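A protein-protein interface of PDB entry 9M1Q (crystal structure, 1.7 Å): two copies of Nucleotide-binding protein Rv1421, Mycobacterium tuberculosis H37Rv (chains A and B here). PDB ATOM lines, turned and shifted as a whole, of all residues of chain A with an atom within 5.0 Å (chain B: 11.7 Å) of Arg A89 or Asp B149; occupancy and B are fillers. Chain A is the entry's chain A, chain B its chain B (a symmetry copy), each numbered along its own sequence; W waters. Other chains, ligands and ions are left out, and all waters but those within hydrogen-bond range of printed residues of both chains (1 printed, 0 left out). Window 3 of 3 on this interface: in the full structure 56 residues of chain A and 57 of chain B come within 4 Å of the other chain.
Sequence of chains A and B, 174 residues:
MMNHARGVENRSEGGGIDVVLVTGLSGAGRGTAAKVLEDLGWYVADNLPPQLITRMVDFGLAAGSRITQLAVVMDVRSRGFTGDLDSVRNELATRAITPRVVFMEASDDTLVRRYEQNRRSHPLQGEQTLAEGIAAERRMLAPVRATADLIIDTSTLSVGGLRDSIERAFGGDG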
ATOM      1  N   LEU A  85     -18.275  22.010 -26.875  1.00  0.00           N
ATOM      2  CA  LEU A  85     -18.020  23.442 -26.994  1.00  0.00           C
ATOM      3  C   LEU A  85     -18.089  23.936 -28.435  1.00  0.00           C
ATOM      4  O   LEU A  85     -17.642  25.054 -28.718  1.00  0.00           O
ATOM      5  CB  LEU A  85     -16.651  23.798 -26.400  1.00  0.00           C
ATOM      6  CG  LEU A  85     -16.498  23.874 -24.878  1.00  0.00           C
ATOM      7  CD1 LEU A  85     -15.043  24.105 -24.504  1.00  0.00           C
ATOM      8  CD2 LEU A  85     -17.366  24.976 -24.299  1.00  0.00           C
ATOM      9  N   ASP A  86     -18.627  23.134 -29.359  1.00  0.00           N
ATOM     10  CA  ASP A  86     -18.675  23.563 -30.755  1.00  0.00           C
ATOM     11  C   ASP A  86     -19.600  24.756 -30.950  1.00  0.00           C
ATOM     12  O   ASP A  86     -19.393  25.553 -31.869  1.00  0.00           O
ATOM     13  CB  ASP A  86     -19.110  22.409 -31.653  1.00  0.00           C
ATOM     14  CG  ASP A  86     -18.149  21.246 -31.603  1.00  0.00           C
ATOM     15  OD1 ASP A  86     -17.308  21.220 -30.679  1.00  0.00           O
ATOM     16  OD2 ASP A  86     -18.227  20.365 -32.485  1.00  0.00           O
ATOM     17  N   SER A  87     -20.621  24.895 -30.104  1.00  0.00           N
ATOM     18  CA  SER A  87     -21.499  26.055 -30.209  1.00  0.00           C
ATOM     19  C   SER A  87     -20.766  27.333 -29.824  1.00  0.00           C
ATOM     20  O   SER A  87     -20.910  28.365 -30.492  1.00  0.00           O
ATOM     21  CB  SER A  87     -22.733  25.855 -29.330  1.00  0.00           C
ATOM     22  OG  SER A  87     -23.711  26.843 -29.591  1.00  0.00           O
ATOM     23  N   VAL A  88     -19.965  27.279 -28.757  1.00  0.00           N
ATOM     24  CA  VAL A  88     -19.250  28.466 -28.304  1.00  0.00           C
ATOM     25  C   VAL A  88     -18.159  28.846 -29.296  1.00  0.00           C
ATOM     26  O   VAL A  88     -17.958  30.030 -29.594  1.00  0.00           O
ATOM     27  CB  VAL A  88     -18.680  28.237 -26.891  1.00  0.00           C
ATOM     28  CG1 VAL A  88     -17.998  29.504 -26.370  1.00  0.00           C
ATOM     29  CG2 VAL A  88     -19.786  27.794 -25.943  1.00  0.00           C
ATOM     30  N   ARG A  89     -17.439  27.855 -29.825  1.00  0.00           N
ATOM     31  CA  ARG A  89     -16.344  28.156 -30.741  1.00  0.00           C
ATOM     32  C   ARG A  89     -16.853  28.803 -32.028  1.00  0.00           C
ATOM     33  O   ARG A  89     -16.249  29.758 -32.530  1.00  0.00           O
ATOM     34  CB  ARG A  89     -15.546  26.888 -31.048  1.00  0.00           C
ATOM     35  CG  ARG A  89     -14.596  26.445 -29.927  1.00  0.00           C
ATOM     36  CD  ARG A  89     -13.637  25.363 -30.417  1.00  0.00           C
ATOM     37  NE  ARG A  89     -12.658  24.944 -29.416  1.00  0.00           N
ATOM     38  CZ  ARG A  89     -11.461  25.497 -29.262  1.00  0.00           C
ATOM     39  NH1 ARG A  89     -11.096  26.555 -29.970  1.00  0.00           N
ATOM     40  NH2 ARG A  89     -10.607  24.972 -28.381  1.00  0.00           N
ATOM     41  N   ASN A  90     -17.967  28.301 -32.570  1.00  0.00           N
ATOM     42  CA  ASN A  90     -18.482  28.839 -33.828  1.00  0.00           C
ATOM     43  C   ASN A  90     -18.988  30.265 -33.657  1.00  0.00           C
ATOM     44  O   ASN A  90     -18.736  31.126 -34.509  1.00  0.00           O
ATOM     45  CB  ASN A  90     -19.588  27.933 -34.376  1.00  0.00           C
ATOM     46  CG  ASN A  90     -19.062  26.587 -34.852  1.00  0.00           C
ATOM     47  OD1 ASN A  90     -17.957  26.496 -35.392  1.00  0.00           O
ATOM     48  ND2 ASN A  90     -19.850  25.536 -34.650  1.00  0.00           N
ATOM     49  N   GLU A  91     -19.692  30.543 -32.557  1.00  0.00           N
ATOM     50  CA  GLU A  91     -20.191  31.896 -32.331  1.00  0.00           C
ATOM     51  C   GLU A  91     -19.054  32.875 -32.051  1.00  0.00           C
ATOM     52  O   GLU A  91     -19.088  34.020 -32.519  1.00  0.00           O
ATOM     53  CB  GLU A  91     -21.208  31.890 -31.194  1.00  0.00           C
ATOM     54  CG  GLU A  91     -22.633  31.633 -31.670  1.00  0.00           C
ATOM     55  CD  GLU A  91     -23.232  32.839 -32.380  1.00  0.00           C
ATOM     56  OE1 GLU A  91     -23.197  33.948 -31.805  1.00  0.00           O
ATOM     57  OE2 GLU A  91     -23.726  32.682 -33.517  1.00  0.00           O
ATOM     58  N   LEU A  92     -18.036  32.453 -31.295  1.00  0.00           N
ATOM     59  CA  LEU A  92     -16.859  33.301 -31.141  1.00  0.00           C
ATOM     60  C   LEU A  92     -16.142  33.507 -32.469  1.00  0.00           C
ATOM     61  O   LEU A  92     -15.557  34.570 -32.701  1.00  0.00           O
ATOM     62  CB  LEU A  92     -15.903  32.700 -30.109  1.00  0.00           C
ATOM     63  CG  LEU A  92     -16.364  32.794 -28.656  1.00  0.00           C
ATOM     64  CD1 LEU A  92     -15.457  31.962 -27.757  1.00  0.00           C
ATOM     65  CD2 LEU A  92     -16.385  34.234 -28.186  1.00  0.00           C
ATOM     66  N   ALA A  93     -16.183  32.502 -33.349  1.00  0.00           N
ATOM     67  CA  ALA A  93     -15.508  32.608 -34.639  1.00  0.00           C
ATOM     68  C   ALA A  93     -16.090  33.738 -35.481  1.00  0.00           C
ATOM     69  O   ALA A  93     -15.356  34.424 -36.203  1.00  0.00           O
ATOM     70  CB  ALA A  93     -15.602  31.279 -35.387  1.00  0.00           C
ATOM     71  N   ILE A  97     -12.571  35.683 -32.876  1.00  0.00           N
ATOM     72  CA  ILE A  97     -12.008  35.229 -31.608  1.00  0.00           C
ATOM     73  C   ILE A  97     -11.898  33.713 -31.641  1.00  0.00           C
ATOM     74  O   ILE A  97     -12.889  33.022 -31.907  1.00  0.00           O
ATOM     75  CB  ILE A  97     -12.866  35.679 -30.409  1.00  0.00           C
ATOM     76  CG1 ILE A  97     -12.871  37.205 -30.313  1.00  0.00           C
ATOM     77  CG2 ILE A  97     -12.353  35.053 -29.102  1.00  0.00           C
ATOM     78  CD1 ILE A  97     -13.945  37.748 -29.415  1.00  0.00           C
ATOM     79  N   THR A  98     -10.696  33.200 -31.375  1.00  0.00           N
ATOM     80  CA  THR A  98     -10.495  31.770 -31.156  1.00  0.00           C
ATOM     81  C   THR A  98     -10.192  31.553 -29.680  1.00  0.00           C
ATOM     82  O   THR A  98      -9.107  31.933 -29.219  1.00  0.00           O
ATOM     83  CB  THR A  98      -9.354  31.220 -32.017  1.00  0.00           C
ATOM     84  OG1 THR A  98      -9.659  31.418 -33.406  1.00  0.00           O
ATOM     85  CG2 THR A  98      -9.178  29.731 -31.754  1.00  0.00           C
ATOM     86  N   PRO A  99     -11.102  30.972 -28.905  1.00  0.00           N
ATOM     87  CA  PRO A  99     -10.826  30.772 -27.480  1.00  0.00           C
ATOM     88  C   PRO A  99      -9.730  29.740 -27.275  1.00  0.00           C
ATOM     89  O   PRO A  99      -9.469  28.884 -28.125  1.00  0.00           O
ATOM     90  CB  PRO A  99     -12.160  30.280 -26.922  1.00  0.00           C
ATOM     91  CG  PRO A  99     -12.803  29.583 -28.086  1.00  0.00           C
ATOM     92  CD  PRO A  99     -12.394  30.392 -29.306  1.00  0.00           C
ATOM     93  N   ARG A 100      -9.075  29.843 -26.127  1.00  0.00           N
ATOM     94  CA  ARG A 100      -8.085  28.862 -25.698  1.00  0.00           C
ATOM     95  C   ARG A 100      -8.684  28.101 -24.526  1.00  0.00           C
ATOM     96  O   ARG A 100      -9.066  28.716 -23.527  1.00  0.00           O
ATOM     97  CB  ARG A 100      -6.777  29.552 -25.325  1.00  0.00           C
ATOM     98  CG  ARG A 100      -6.099  30.199 -26.539  1.00  0.00           C
ATOM     99  CD  ARG A 100      -4.726  30.729 -26.178  1.00  0.00           C
ATOM    100  NE  ARG A 100      -4.814  31.956 -25.400  1.00  0.00           N
ATOM    101  CZ  ARG A 100      -3.905  32.345 -24.517  1.00  0.00           C
ATOM    102  NH1 ARG A 100      -2.849  31.597 -24.238  1.00  0.00           N
ATOM    103  NH2 ARG A 100      -4.062  33.507 -23.893  1.00  0.00           N
ATOM    104  N   VAL A 101      -8.804  26.781 -24.663  1.00  0.00           N
ATOM    105  CA  VAL A 101      -9.472  25.940 -23.663  1.00  0.00           C
ATOM    106  C   VAL A 101      -8.429  25.219 -22.815  1.00  0.00           C
ATOM    107  O   VAL A 101      -7.580  24.484 -23.338  1.00  0.00           O
ATOM    108  CB  VAL A 101     -10.428  24.937 -24.327  1.00  0.00           C
ATOM    109  CG1 VAL A 101     -11.017  23.980 -23.290  1.00  0.00           C
ATOM    110  CG2 VAL A 101     -11.530  25.695 -25.125  1.00  0.00           C
ATOM    111  N   LEU B 141     -17.261  15.318 -19.338  1.00  0.00           N
ATOM    112  CA  LEU B 141     -16.297  16.294 -19.836  1.00  0.00           C
ATOM    113  C   LEU B 141     -15.432  15.767 -20.977  1.00  0.00           C
ATOM    114  O   LEU B 141     -14.602  16.528 -21.506  1.00  0.00           O
ATOM    115  CB  LEU B 141     -15.403  16.769 -18.690  1.00  0.00           C
ATOM    116  CG  LEU B 141     -16.122  17.700 -17.703  1.00  0.00           C
ATOM    117  CD1 LEU B 141     -15.237  17.961 -16.518  1.00  0.00           C
ATOM    118  CD2 LEU B 141     -16.530  18.995 -18.367  1.00  0.00           C
ATOM    119  N   ALA B 142     -15.613  14.508 -21.376  1.00  0.00           N
ATOM    120  CA  ALA B 142     -14.792  13.940 -22.445  1.00  0.00           C
ATOM    121  C   ALA B 142     -14.811  14.762 -23.734  1.00  0.00           C
ATOM    122  O   ALA B 142     -13.728  14.951 -24.321  1.00  0.00           O
ATOM    123  CB  ALA B 142     -15.206  12.480 -22.709  1.00  0.00           C
ATOM    124  N   PRO B 143     -15.950  15.281 -24.225  1.00  0.00           N
ATOM    125  CA  PRO B 143     -15.883  16.113 -25.447  1.00  0.00           C
ATOM    126  C   PRO B 143     -15.106  17.402 -25.246  1.00  0.00           C
ATOM    127  O   PRO B 143     -14.395  17.849 -26.157  1.00  0.00           O
ATOM    128  CB  PRO B 143     -17.361  16.388 -25.776  1.00  0.00           C
ATOM    129  CG  PRO B 143     -18.125  15.311 -25.078  1.00  0.00           C
ATOM    130  CD  PRO B 143     -17.348  15.044 -23.812  1.00  0.00           C
ATOM    131  N   VAL B 144     -15.217  18.017 -24.071  1.00  0.00           N
ATOM    132  CA  VAL B 144     -14.455  19.235 -23.818  1.00  0.00           C
ATOM    133  C   VAL B 144     -12.967  18.922 -23.743  1.00  0.00           C
ATOM    134  O   VAL B 144     -12.135  19.672 -24.274  1.00  0.00           O
ATOM    135  CB  VAL B 144     -14.955  19.929 -22.535  1.00  0.00           C
ATOM    136  CG1 VAL B 144     -14.087  21.128 -22.223  1.00  0.00           C
ATOM    137  CG2 VAL B 144     -16.392  20.374 -22.701  1.00  0.00           C
ATOM    138  N   ARG B 145     -12.606  17.825 -23.070  1.00  0.00           N
ATOM    139  CA  ARG B 145     -11.203  17.448 -22.971  1.00  0.00           C
ATOM    140  C   ARG B 145     -10.610  17.228 -24.352  1.00  0.00           C
ATOM    141  O   ARG B 145      -9.473  17.644 -24.628  1.00  0.00           O
ATOM    142  CB  ARG B 145     -11.057  16.187 -22.127  1.00  0.00           C
ATOM    143  CG  ARG B 145      -9.608  15.830 -21.802  1.00  0.00           C
ATOM    144  CD  ARG B 145      -9.486  14.469 -21.153  1.00  0.00           C
ATOM    145  NE  ARG B 145      -8.143  14.219 -20.641  1.00  0.00           N
ATOM    146  CZ  ARG B 145      -7.111  13.844 -21.386  1.00  0.00           C
ATOM    147  NH1 ARG B 145      -7.239  13.627 -22.687  1.00  0.00           N
ATOM    148  NH2 ARG B 145      -5.909  13.717 -20.820  1.00  0.00           N
ATOM    149  N   ALA B 146     -11.386  16.591 -25.240  1.00  0.00           N
ATOM    150  CA  ALA B 146     -10.917  16.258 -26.583  1.00  0.00           C
ATOM    151  C   ALA B 146     -10.697  17.488 -27.452  1.00  0.00           C
ATOM    152  O   ALA B 146     -10.049  17.382 -28.498  1.00  0.00           O
ATOM    153  CB  ALA B 146     -11.920  15.312 -27.252  1.00  0.00           C
ATOM    154  N   THR B 147     -11.228  18.646 -27.062  1.00  0.00           N
ATOM    155  CA  THR B 147     -11.013  19.889 -27.789  1.00  0.00           C
ATOM    156  C   THR B 147     -10.105  20.861 -27.046  1.00  0.00           C
ATOM    157  O   THR B 147      -9.959  22.001 -27.476  1.00  0.00           O
ATOM    158  CB  THR B 147     -12.345  20.580 -28.092  1.00  0.00           C
ATOM    159  OG1 THR B 147     -12.113  21.664 -29.007  1.00  0.00           O
ATOM    160  CG2 THR B 147     -12.951  21.178 -26.827  1.00  0.00           C
ATOM    161  N   ALA B 148      -9.515  20.459 -25.927  1.00  0.00           N
ATOM    162  CA  ALA B 148      -8.751  21.417 -25.144  1.00  0.00           C
ATOM    163  C   ALA B 148      -7.406  21.707 -25.803  1.00  0.00           C
ATOM    164  O   ALA B 148      -6.774  20.818 -26.385  1.00  0.00           O
ATOM    165  CB  ALA B 148      -8.534  20.898 -23.723  1.00  0.00           C
ATOM    166  N   ASP B 149      -6.960  22.950 -25.677  1.00  0.00           N
ATOM    167  CA  ASP B 149      -5.650  23.358 -26.178  1.00  0.00           C
ATOM    168  C   ASP B 149      -4.550  22.987 -25.198  1.00  0.00           C
ATOM    169  O   ASP B 149      -3.402  22.765 -25.593  1.00  0.00           O
ATOM    170  CB  ASP B 149      -5.632  24.868 -26.416  1.00  0.00           C
ATOM    171  CG  ASP B 149      -6.660  25.303 -27.433  1.00  0.00           C
ATOM    172  OD1 ASP B 149      -6.382  25.175 -28.650  1.00  0.00           O
ATOM    173  OD2 ASP B 149      -7.776  25.724 -27.038  1.00  0.00           O
ATOM    174  N   LEU B 150      -4.876  22.942 -23.909  1.00  0.00           N
ATOM    175  CA  LEU B 150      -3.886  22.695 -22.868  1.00  0.00           C
ATOM    176  C   LEU B 150      -4.543  21.819 -21.814  1.00  0.00           C
ATOM    177  O   LEU B 150      -5.619  22.166 -21.312  1.00  0.00           O
ATOM    178  CB  LEU B 150      -3.395  24.000 -22.240  1.00  0.00           C
ATOM    179  CG  LEU B 150      -2.479  23.888 -21.008  1.00  0.00           C
ATOM    180  CD1 LEU B 150      -1.199  23.074 -21.313  1.00  0.00           C
ATOM    181  CD2 LEU B 150      -2.143  25.293 -20.456  1.00  0.00           C
ATOM    182  N   ILE B 151      -3.926  20.687 -21.495  1.00  0.00           N
ATOM    183  CA  ILE B 151      -4.406  19.816 -20.426  1.00  0.00           C
ATOM    184  C   ILE B 151      -3.364  19.831 -19.328  1.00  0.00           C
ATOM    185  O   ILE B 151      -2.175  19.585 -19.578  1.00  0.00           O
ATOM    186  CB  ILE B 151      -4.680  18.389 -20.924  1.00  0.00           C
ATOM    187  CG1 ILE B 151      -5.772  18.434 -21.988  1.00  0.00           C
ATOM    188  CG2 ILE B 151      -5.031  17.467 -19.743  1.00  0.00           C
ATOM    189  CD1 ILE B 151      -6.144  17.071 -22.612  1.00  0.00           C
ATOM    190  N   ILE B 152      -3.783  20.159 -18.108  1.00  0.00           N
ATOM    191  CA  ILE B 152      -2.851  20.225 -16.986  1.00  0.00           C
ATOM    192  C   ILE B 152      -3.221  19.110 -16.032  1.00  0.00           C
ATOM    193  O   ILE B 152      -4.319  19.121 -15.461  1.00  0.00           O
ATOM    194  CB  ILE B 152      -2.880  21.589 -16.267  1.00  0.00           C
ATOM    195  CG1 ILE B 152      -2.611  22.732 -17.255  1.00  0.00           C
ATOM    196  CG2 ILE B 152      -1.828  21.576 -15.156  1.00  0.00           C
ATOM    197  CD1 ILE B 152      -2.698  24.158 -16.651  1.00  0.00           C
ATOM    198  N   ASP B 153      -2.309  18.142 -15.870  1.00  0.00           N
ATOM    199  CA  ASP B 153      -2.494  17.001 -14.985  1.00  0.00           C
ATOM    200  C   ASP B 153      -1.821  17.329 -13.657  1.00  0.00           C
ATOM    201  O   ASP B 153      -0.593  17.469 -13.596  1.00  0.00           O
ATOM    202  CB  ASP B 153      -1.900  15.746 -15.625  1.00  0.00           C
ATOM    203  CG  ASP B 153      -2.081  14.500 -14.792  1.00  0.00           C
ATOM    204  OD1 ASP B 153      -2.379  14.548 -13.578  1.00  0.00           O
ATOM    205  OD2 ASP B 153      -1.920  13.412 -15.374  1.00  0.00           O
ATOM    206  N   ALA B 169       2.798  26.215 -16.770  1.00  0.00           N
ATOM    207  CA  ALA B 169       1.992  25.920 -17.950  1.00  0.00           C
ATOM    208  C   ALA B 169       1.495  27.184 -18.640  1.00  0.00           C
ATOM    209  O   ALA B 169       1.350  27.197 -19.872  1.00  0.00           O
ATOM    210  CB  ALA B 169       0.815  25.023 -17.555  1.00  0.00           C
ATOM    211  N   PHE B 170       1.221  28.249 -17.886  1.00  0.00           N
ATOM    212  CA  PHE B 170       0.690  29.474 -18.468  1.00  0.00           C
ATOM    213  C   PHE B 170       1.781  30.443 -18.892  1.00  0.00           C
ATOM    214  O   PHE B 170       1.458  31.537 -19.363  1.00  0.00           O
ATOM    215  CB  PHE B 170      -0.253  30.206 -17.506  1.00  0.00           C
ATOM    216  CG  PHE B 170      -1.587  29.545 -17.313  1.00  0.00           C
ATOM    217  CD1 PHE B 170      -1.973  28.461 -18.090  1.00  0.00           C
ATOM    218  CD2 PHE B 170      -2.464  30.009 -16.344  1.00  0.00           C
ATOM    219  CE1 PHE B 170      -3.199  27.847 -17.885  1.00  0.00           C
ATOM    220  CE2 PHE B 170      -3.690  29.410 -16.139  1.00  0.00           C
ATOM    221  CZ  PHE B 170      -4.069  28.334 -16.909  1.00  0.00           C
HETATM  222  O   HOH W   1      -7.621  27.330 -29.750  1.00  0.00           O
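The backbone carbonyl oxygen (O) of Thr B147 sits at hydrogen-bond distance from the guanidinium group (NH2) of Arg A89 (3.2 Å). The side-chain carboxylate of Asp B149 is in salt-bridge range of the guanidinium group of Arg A89 (3.2 Å). The side-chain carboxylate of Asp B149 is in hydrogen-bond range of the backbone NH of Val A101 (2.8 Å). The backbone carbonyl oxygen (O) of Val A101 sits at hydrogen-bond distance from the backbone NH (N) of Leu B150, at 3.2 Å.
NH1 of Arg A89 lies within hydrogen-bond range of O of Pro A99, at 3.4 Å.
Among the printed residues, pairs that only touch across the chains: Leu A85 with Val B144 (3.9 Å), Pro A99 with Asp B149 (3.7 Å), Arg A100 with Asp B149 (3.4 Å) and Val A101 with Ala B148 (3.7 Å).
Of chain B, only Thr B147 and Asp B149 come within 4 Å of Arg A89. Asp B149 touches just these residues of chain A: Arg A89 (3.2 Å), Pro A99 (3.7 Å), Arg A100 (3.4 Å) and Val A101 (2.8 Å). Of chain B, only Val B144 comes within 4 Å of Leu A85. No residue of chain B comes within 4 Å of Asp A86. Ser A87 touches none of the printed residues of chain B. No residue of chain B comes within 4 Å of Val A88. No residue of chain B comes within 4 Å of Asn A90. No residue of chain B comes within 4 Å of Ala A93. Of chain B, only Asp B149 (3.7 Å) comes within 4 Å of Pro A99. Of chain B, only Ala B148 (3.7 Å), Asp B149 (2.8 Å) and Leu B150 (3.2 Å) come within 4 Å of Val A101. Printed residues of chain B within 4 Å of Arg A100: Asp B149 (3.4 Å). Of the printed residues of chain A, Val B144 touches Leu A85 (3.9 Å). Of the printed residues of chain A, Leu B150 touches Val A101 (3.2 Å). Ala B142 touches none of the printed residues of chain A. The nearest residue of chain B that does not touch Arg A89 is Ala B148 (5.2 Å). The nearest printed residue of chain A that does not touch Asp B149 is Thr A98 (6.2 Å).
Hydrophobic or aromatic side chains of chain A that line the printed part of chain B: Leu A85 and Val A101. Of the 15 printed residues of chain B, 5 touch a printed residue of chain A. Hydrophobic or aromatic side chains of chain B within 4 Å of the printed part of chain A: Val B144 and Ala B148.
No position is printed for both chains. Of the 8 pairs that touch across the chains among the printed residues, none has its exchanged pair printed and touching as well.
Water W1 lies within hydrogen-bond range of the side-chain carboxylate (OD1) of Asp B149 (2.7 Å) and the backbone carbonyl oxygen (O) of Pro A99 (2.9 Å).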
